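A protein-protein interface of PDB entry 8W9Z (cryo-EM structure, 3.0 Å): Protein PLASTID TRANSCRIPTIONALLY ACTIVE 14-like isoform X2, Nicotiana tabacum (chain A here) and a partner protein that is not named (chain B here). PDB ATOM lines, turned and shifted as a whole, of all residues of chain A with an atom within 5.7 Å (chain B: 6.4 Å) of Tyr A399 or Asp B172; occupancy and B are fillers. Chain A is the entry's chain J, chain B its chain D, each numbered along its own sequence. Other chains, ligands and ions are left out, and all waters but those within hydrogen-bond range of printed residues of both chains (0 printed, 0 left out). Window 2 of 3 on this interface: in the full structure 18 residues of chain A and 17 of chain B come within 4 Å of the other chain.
Of chain B, only Asp B172 comes within 4 Å of Tyr A399. Of chain A, only Ser A392, Gly A393 and Tyr A399 come within 4 Å of Asp B172. Printed residues of chain B within 4 Å of Asn A401: Lys B170 (3.6 Å). Of the printed residues of chain B, Gly A393 touches Asp B172 (3.7 Å) and Gln B175 (3.99 Å). Of the printed residues of chain A, Gln B175 touches Gly A393 (3.99 Å). Of the printed residues of chain A, Lys B170 touches Asn A401. His B140 touches none of the printed residues of chain A. Ile A417 touches none of the printed residues of chain B. The nearest residue of chain B that does not touch Tyr A399 is Tyr B171 (5.7 Å). The nearest printed residue of chain B that does not touch Gly A393 is His B140 (6.6 Å).
Asp B172 touches Ser A392. N of Gly A393 touches OD2 of Asp B172, at 3.7 Å. O of Gly A393 touches NE2 of Gln B175, 3.99 Å away. Tyr A399 touches Asp B172 (OH to CB, 3.6 Å). Lys B170 touches Asn A401 (O to ND2, 3.6 Å).
Of the 10 printed residues of chain B, 3 touch a printed residue of chain A. Printed residues of chain B that touch a printed residue of chain A: Lys B170, Asp B172 and Gln B175.
O of Asn A390 lies within hydrogen-bond range of N of Asn A401, at 3.1 Å. The backbone NH (N) of Ser A392 is in hydrogen-bond range of the backbone carbonyl oxygen (O) of Tyr A399 (3.4 Å). The side-chain hydroxyl (OG) of Ser A392 sits at hydrogen-bond distance from the side-chain amide nitrogen (ND2) of Asn A401 (3.4 Å).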
ATOM      1  N   ASN A 390     -20.732  25.223   5.318  1.00  0.00           N
ATOM      2  CA  ASN A 390     -19.775  24.889   6.374  1.00  0.00           C
ATOM      3  C   ASN A 390     -20.389  23.988   7.442  1.00  0.00           C
ATOM      4  O   ASN A 390     -20.016  24.056   8.615  1.00  0.00           O
ATOM      5  CB  ASN A 390     -19.191  26.153   7.013  1.00  0.00           C
ATOM      6  CG  ASN A 390     -18.414  26.999   6.027  1.00  0.00           C
ATOM      7  OD1 ASN A 390     -18.798  28.129   5.723  1.00  0.00           O
ATOM      8  ND2 ASN A 390     -17.313  26.457   5.520  1.00  0.00           N
ATOM      9  N   ILE A 391     -21.335  23.138   7.046  1.00  0.00           N
ATOM     10  CA  ILE A 391     -21.973  22.197   7.969  1.00  0.00           C
ATOM     11  C   ILE A 391     -21.153  20.913   7.903  1.00  0.00           C
ATOM     12  O   ILE A 391     -21.387  20.037   7.071  1.00  0.00           O
ATOM     13  CB  ILE A 391     -23.444  21.969   7.632  1.00  0.00           C
ATOM     14  CG1 ILE A 391     -24.205  23.296   7.637  1.00  0.00           C
ATOM     15  CG2 ILE A 391     -24.073  21.003   8.620  1.00  0.00           C
ATOM     16  CD1 ILE A 391     -25.672  23.156   7.302  1.00  0.00           C
ATOM     17  N   SER A 392     -20.170  20.805   8.793  1.00  0.00           N
ATOM     18  CA  SER A 392     -19.277  19.657   8.841  1.00  0.00           C
ATOM     19  C   SER A 392     -19.673  18.743   9.991  1.00  0.00           C
ATOM     20  O   SER A 392     -19.915  19.211  11.107  1.00  0.00           O
ATOM     21  CB  SER A 392     -17.824  20.106   8.998  1.00  0.00           C
ATOM     22  OG  SER A 392     -17.645  20.846  10.194  1.00  0.00           O
ATOM     23  N   GLY A 393     -19.738  17.453   9.716  1.00  0.00           N
ATOM     24  CA  GLY A 393     -20.062  16.473  10.735  1.00  0.00           C
ATOM     25  C   GLY A 393     -20.813  15.302  10.140  1.00  0.00           C
ATOM     26  O   GLY A 393     -21.242  15.318   8.989  1.00  0.00           O
ATOM     27  N   GLU A 397     -24.789  14.229  13.834  1.00  0.00           N
ATOM     28  CA  GLU A 397     -24.374  15.449  14.523  1.00  0.00           C
ATOM     29  C   GLU A 397     -23.847  16.438  13.486  1.00  0.00           C
ATOM     30  O   GLU A 397     -22.723  16.297  12.997  1.00  0.00           O
ATOM     31  CB  GLU A 397     -23.324  15.143  15.588  1.00  0.00           C
ATOM     32  CG  GLU A 397     -23.051  16.287  16.554  1.00  0.00           C
ATOM     33  CD  GLU A 397     -22.000  17.253  16.044  1.00  0.00           C
ATOM     34  OE1 GLU A 397     -21.129  16.825  15.258  1.00  0.00           O
ATOM     35  OE2 GLU A 397     -22.045  18.440  16.429  1.00  0.00           O
ATOM     36  N   TYR A 398     -24.665  17.432  13.152  1.00  0.00           N
ATOM     37  CA  TYR A 398     -24.287  18.507  12.246  1.00  0.00           C
ATOM     38  C   TYR A 398     -24.020  19.769  13.053  1.00  0.00           C
ATOM     39  O   TYR A 398     -24.850  20.170  13.875  1.00  0.00           O
ATOM     40  CB  TYR A 398     -25.384  18.773  11.214  1.00  0.00           C
ATOM     41  CG  TYR A 398     -25.437  17.784  10.074  1.00  0.00           C
ATOM     42  CD1 TYR A 398     -24.301  17.110   9.659  1.00  0.00           C
ATOM     43  CD2 TYR A 398     -26.627  17.534   9.407  1.00  0.00           C
ATOM     44  CE1 TYR A 398     -24.349  16.210   8.612  1.00  0.00           C
ATOM     45  CE2 TYR A 398     -26.685  16.635   8.362  1.00  0.00           C
ATOM     46  CZ  TYR A 398     -25.545  15.978   7.968  1.00  0.00           C
ATOM     47  OH  TYR A 398     -25.601  15.081   6.927  1.00  0.00           O
ATOM     48  N   TYR A 399     -22.912  20.422  12.816  1.00  0.00           N
ATOM     49  CA  TYR A 399     -22.581  21.594  13.548  1.00  0.00           C
ATOM     50  C   TYR A 399     -22.040  22.556  12.593  1.00  0.00           C
ATOM     51  O   TYR A 399     -21.573  22.159  11.537  1.00  0.00           O
ATOM     52  CB  TYR A 399     -21.558  21.272  14.604  1.00  0.00           C
ATOM     53  CG  TYR A 399     -20.134  20.923  14.270  1.00  0.00           C
ATOM     54  CD1 TYR A 399     -19.726  19.614  14.225  1.00  0.00           C
ATOM     55  CD2 TYR A 399     -19.174  21.903  14.124  1.00  0.00           C
ATOM     56  CE1 TYR A 399     -18.420  19.287  13.953  1.00  0.00           C
ATOM     57  CE2 TYR A 399     -17.868  21.588  13.847  1.00  0.00           C
ATOM     58  CZ  TYR A 399     -17.498  20.275  13.768  1.00  0.00           C
ATOM     59  OH  TYR A 399     -16.192  19.950  13.500  1.00  0.00           O
ATOM     60  N   HIS A 400     -22.077  23.821  12.878  1.00  0.00           N
ATOM     61  CA  HIS A 400     -21.431  24.720  11.957  1.00  0.00           C
ATOM     62  C   HIS A 400     -20.052  24.985  12.374  1.00  0.00           C
ATOM     63  O   HIS A 400     -19.782  25.240  13.543  1.00  0.00           O
ATOM     64  CB  HIS A 400     -22.195  25.959  11.784  1.00  0.00           C
ATOM     65  CG  HIS A 400     -21.423  27.225  11.968  1.00  0.00           C
ATOM     66  ND1 HIS A 400     -20.617  27.759  10.985  1.00  0.00           N
ATOM     67  CD2 HIS A 400     -21.403  28.111  12.992  1.00  0.00           C
ATOM     68  CE1 HIS A 400     -20.113  28.902  11.408  1.00  0.00           C
ATOM     69  NE2 HIS A 400     -20.565  29.134  12.626  1.00  0.00           N
ATOM     70  N   ASN A 401     -19.120  24.868  11.456  1.00  0.00           N
ATOM     71  CA  ASN A 401     -17.744  24.992  11.830  1.00  0.00           C
ATOM     72  C   ASN A 401     -17.411  26.412  11.697  1.00  0.00           C
ATOM     73  O   ASN A 401     -17.327  26.926  10.587  1.00  0.00           O
ATOM     74  CB  ASN A 401     -16.881  24.194  10.886  1.00  0.00           C
ATOM     75  CG  ASN A 401     -15.643  23.654  11.545  1.00  0.00           C
ATOM     76  OD1 ASN A 401     -15.328  23.999  12.683  1.00  0.00           O
ATOM     77  ND2 ASN A 401     -14.928  22.795  10.835  1.00  0.00           N
ATOM     78  N   SER A 402     -17.209  27.086  12.800  1.00  0.00           N
ATOM     79  CA  SER A 402     -16.989  28.493  12.722  1.00  0.00           C
ATOM     80  C   SER A 402     -15.633  28.820  12.253  1.00  0.00           C
ATOM     81  O   SER A 402     -15.438  29.793  11.547  1.00  0.00           O
ATOM     82  CB  SER A 402     -17.206  29.130  14.079  1.00  0.00           C
ATOM     83  OG  SER A 402     -16.185  30.067  14.372  1.00  0.00           O
ATOM     84  N   ILE A 417     -29.522  23.800   9.251  1.00  0.00           N
ATOM     85  CA  ILE A 417     -29.205  22.420   9.612  1.00  0.00           C
ATOM     86  C   ILE A 417     -30.432  21.533   9.442  1.00  0.00           C
ATOM     87  O   ILE A 417     -30.360  20.442   8.862  1.00  0.00           O
ATOM     88  CB  ILE A 417     -28.659  22.354  11.051  1.00  0.00           C
ATOM     89  CG1 ILE A 417     -27.362  23.151  11.169  1.00  0.00           C
ATOM     90  CG2 ILE A 417     -28.442  20.912  11.472  1.00  0.00           C
ATOM     91  CD1 ILE A 417     -26.745  23.104  12.547  1.00  0.00           C
ATOM     92  N   HIS B 140     -13.770  20.130   1.288  1.00  0.00           N
ATOM     93  CA  HIS B 140     -13.803  18.893   2.058  1.00  0.00           C
ATOM     94  C   HIS B 140     -14.013  17.677   1.166  1.00  0.00           C
ATOM     95  O   HIS B 140     -13.463  16.605   1.445  1.00  0.00           O
ATOM     96  CB  HIS B 140     -14.898  18.964   3.121  1.00  0.00           C
ATOM     97  CG  HIS B 140     -14.947  17.769   4.021  1.00  0.00           C
ATOM     98  ND1 HIS B 140     -15.684  16.643   3.723  1.00  0.00           N
ATOM     99  CD2 HIS B 140     -14.351  17.525   5.212  1.00  0.00           C
ATOM    100  CE1 HIS B 140     -15.540  15.757   4.691  1.00  0.00           C
ATOM    101  NE2 HIS B 140     -14.736  16.266   5.607  1.00  0.00           N
ATOM    102  N   MET B 166      -5.572  18.258   6.336  1.00  0.00           N
ATOM    103  CA  MET B 166      -6.924  18.682   6.686  1.00  0.00           C
ATOM    104  C   MET B 166      -6.960  19.294   8.080  1.00  0.00           C
ATOM    105  O   MET B 166      -7.691  20.261   8.322  1.00  0.00           O
ATOM    106  CB  MET B 166      -7.891  17.502   6.599  1.00  0.00           C
ATOM    107  CG  MET B 166      -8.036  16.908   5.213  1.00  0.00           C
ATOM    108  SD  MET B 166      -9.140  15.483   5.195  1.00  0.00           S
ATOM    109  CE  MET B 166     -10.660  16.225   5.780  1.00  0.00           C
ATOM    110  N   GLU B 167      -6.179  18.741   9.009  1.00  0.00           N
ATOM    111  CA  GLU B 167      -6.164  19.257  10.372  1.00  0.00           C
ATOM    112  C   GLU B 167      -5.559  20.655  10.430  1.00  0.00           C
ATOM    113  O   GLU B 167      -6.052  21.519  11.165  1.00  0.00           O
ATOM    114  CB  GLU B 167      -5.400  18.302  11.288  1.00  0.00           C
ATOM    115  CG  GLU B 167      -5.340  18.742  12.744  1.00  0.00           C
ATOM    116  CD  GLU B 167      -6.695  18.705  13.427  1.00  0.00           C
ATOM    117  OE1 GLU B 167      -7.587  17.971  12.953  1.00  0.00           O
ATOM    118  OE2 GLU B 167      -6.868  19.413  14.441  1.00  0.00           O
ATOM    119  N   LYS B 170      -7.895  23.640   9.690  1.00  0.00           N
ATOM    120  CA  LYS B 170      -9.011  23.851  10.614  1.00  0.00           C
ATOM    121  C   LYS B 170     -10.258  23.073  10.201  1.00  0.00           C
ATOM    122  O   LYS B 170     -11.384  23.499  10.466  1.00  0.00           O
ATOM    123  CB  LYS B 170      -9.335  25.341  10.764  1.00  0.00           C
ATOM    124  CG  LYS B 170      -8.165  26.177  11.249  1.00  0.00           C
ATOM    125  CD  LYS B 170      -7.618  25.646  12.562  1.00  0.00           C
ATOM    126  CE  LYS B 170      -6.407  26.440  13.019  1.00  0.00           C
ATOM    127  NZ  LYS B 170      -5.862  25.926  14.306  1.00  0.00           N
ATOM    128  N   TYR B 171     -10.070  21.927   9.551  1.00  0.00           N
ATOM    129  CA  TYR B 171     -11.180  21.051   9.214  1.00  0.00           C
ATOM    130  C   TYR B 171     -11.450  20.076  10.359  1.00  0.00           C
ATOM    131  O   TYR B 171     -10.866  20.162  11.443  1.00  0.00           O
ATOM    132  CB  TYR B 171     -10.890  20.292   7.923  1.00  0.00           C
ATOM    133  CG  TYR B 171     -11.328  20.999   6.660  1.00  0.00           C
ATOM    134  CD1 TYR B 171     -10.521  21.953   6.058  1.00  0.00           C
ATOM    135  CD2 TYR B 171     -12.543  20.696   6.062  1.00  0.00           C
ATOM    136  CE1 TYR B 171     -10.916  22.594   4.901  1.00  0.00           C
ATOM    137  CE2 TYR B 171     -12.946  21.332   4.904  1.00  0.00           C
ATOM    138  CZ  TYR B 171     -12.129  22.279   4.328  1.00  0.00           C
ATOM    139  OH  TYR B 171     -12.527  22.916   3.175  1.00  0.00           O
ATOM    140  N   ASP B 172     -12.357  19.135  10.113  1.00  0.00           N
ATOM    141  CA  ASP B 172     -12.631  18.032  11.023  1.00  0.00           C
ATOM    142  C   ASP B 172     -12.196  16.733  10.359  1.00  0.00           C
ATOM    143  O   ASP B 172     -12.542  16.479   9.201  1.00  0.00           O
ATOM    144  CB  ASP B 172     -14.113  17.978  11.395  1.00  0.00           C
ATOM    145  CG  ASP B 172     -15.018  17.923  10.180  1.00  0.00           C
ATOM    146  OD1 ASP B 172     -14.646  18.492   9.133  1.00  0.00           O
ATOM    147  OD2 ASP B 172     -16.103  17.310  10.273  1.00  0.00           O
ATOM    148  N   ILE B 173     -11.437  15.919  11.089  1.00  0.00           N
ATOM    149  CA  ILE B 173     -10.833  14.726  10.509  1.00  0.00           C
ATOM    150  C   ILE B 173     -11.505  13.470  11.045  1.00  0.00           C
ATOM    151  O   ILE B 173     -10.883  12.403  11.108  1.00  0.00           O
ATOM    152  CB  ILE B 173      -9.317  14.690  10.776  1.00  0.00           C
ATOM    153  CG1 ILE B 173      -9.037  14.753  12.279  1.00  0.00           C
ATOM    154  CG2 ILE B 173      -8.622  15.831  10.051  1.00  0.00           C
ATOM    155  CD1 ILE B 173      -7.570  14.658  12.629  1.00  0.00           C
ATOM    156  N   ARG B 174     -12.775  13.578  11.435  1.00  0.00           N
ATOM    157  CA  ARG B 174     -13.487  12.408  11.939  1.00  0.00           C
ATOM    158  C   ARG B 174     -14.025  11.554  10.796  1.00  0.00           C
ATOM    159  O   ARG B 174     -13.687  10.369  10.677  1.00  0.00           O
ATOM    160  CB  ARG B 174     -14.624  12.839  12.869  1.00  0.00           C
ATOM    161  CG  ARG B 174     -15.401  11.674  13.456  1.00  0.00           C
ATOM    162  CD  ARG B 174     -16.527  12.147  14.357  1.00  0.00           C
ATOM    163  NE  ARG B 174     -17.317  11.030  14.866  1.00  0.00           N
ATOM    164  CZ  ARG B 174     -18.369  11.162  15.663  1.00  0.00           C
ATOM    165  NH1 ARG B 174     -18.765  12.367  16.049  1.00  0.00           N
ATOM    166  NH2 ARG B 174     -19.029  10.088  16.076  1.00  0.00           N
ATOM    167  N   GLN B 175     -14.867  12.143   9.944  1.00  0.00           N
ATOM    168  CA  GLN B 175     -15.456  11.385   8.845  1.00  0.00           C
ATOM    169  C   GLN B 175     -14.393  10.915   7.863  1.00  0.00           C
ATOM    170  O   GLN B 175     -14.492   9.812   7.313  1.00  0.00           O
ATOM    171  CB  GLN B 175     -16.511  12.227   8.131  1.00  0.00           C
ATOM    172  CG  GLN B 175     -17.256  11.480   7.038  1.00  0.00           C
ATOM    173  CD  GLN B 175     -18.325  12.323   6.378  1.00  0.00           C
ATOM    174  OE1 GLN B 175     -19.063  11.846   5.517  1.00  0.00           O
ATOM    175  NE2 GLN B 175     -18.412  13.586   6.776  1.00  0.00           N
ATOM    176  N   ALA B 176     -13.362  11.732   7.635  1.00  0.00           N
ATOM    177  CA  ALA B 176     -12.277  11.316   6.755  1.00  0.00           C
ATOM    178  C   ALA B 176     -11.534  10.118   7.330  1.00  0.00           C
ATOM    179  O   ALA B 176     -11.186   9.184   6.600  1.00  0.00           O
ATOM    180  CB  ALA B 176     -11.318  12.481   6.514  1.00  0.00           C
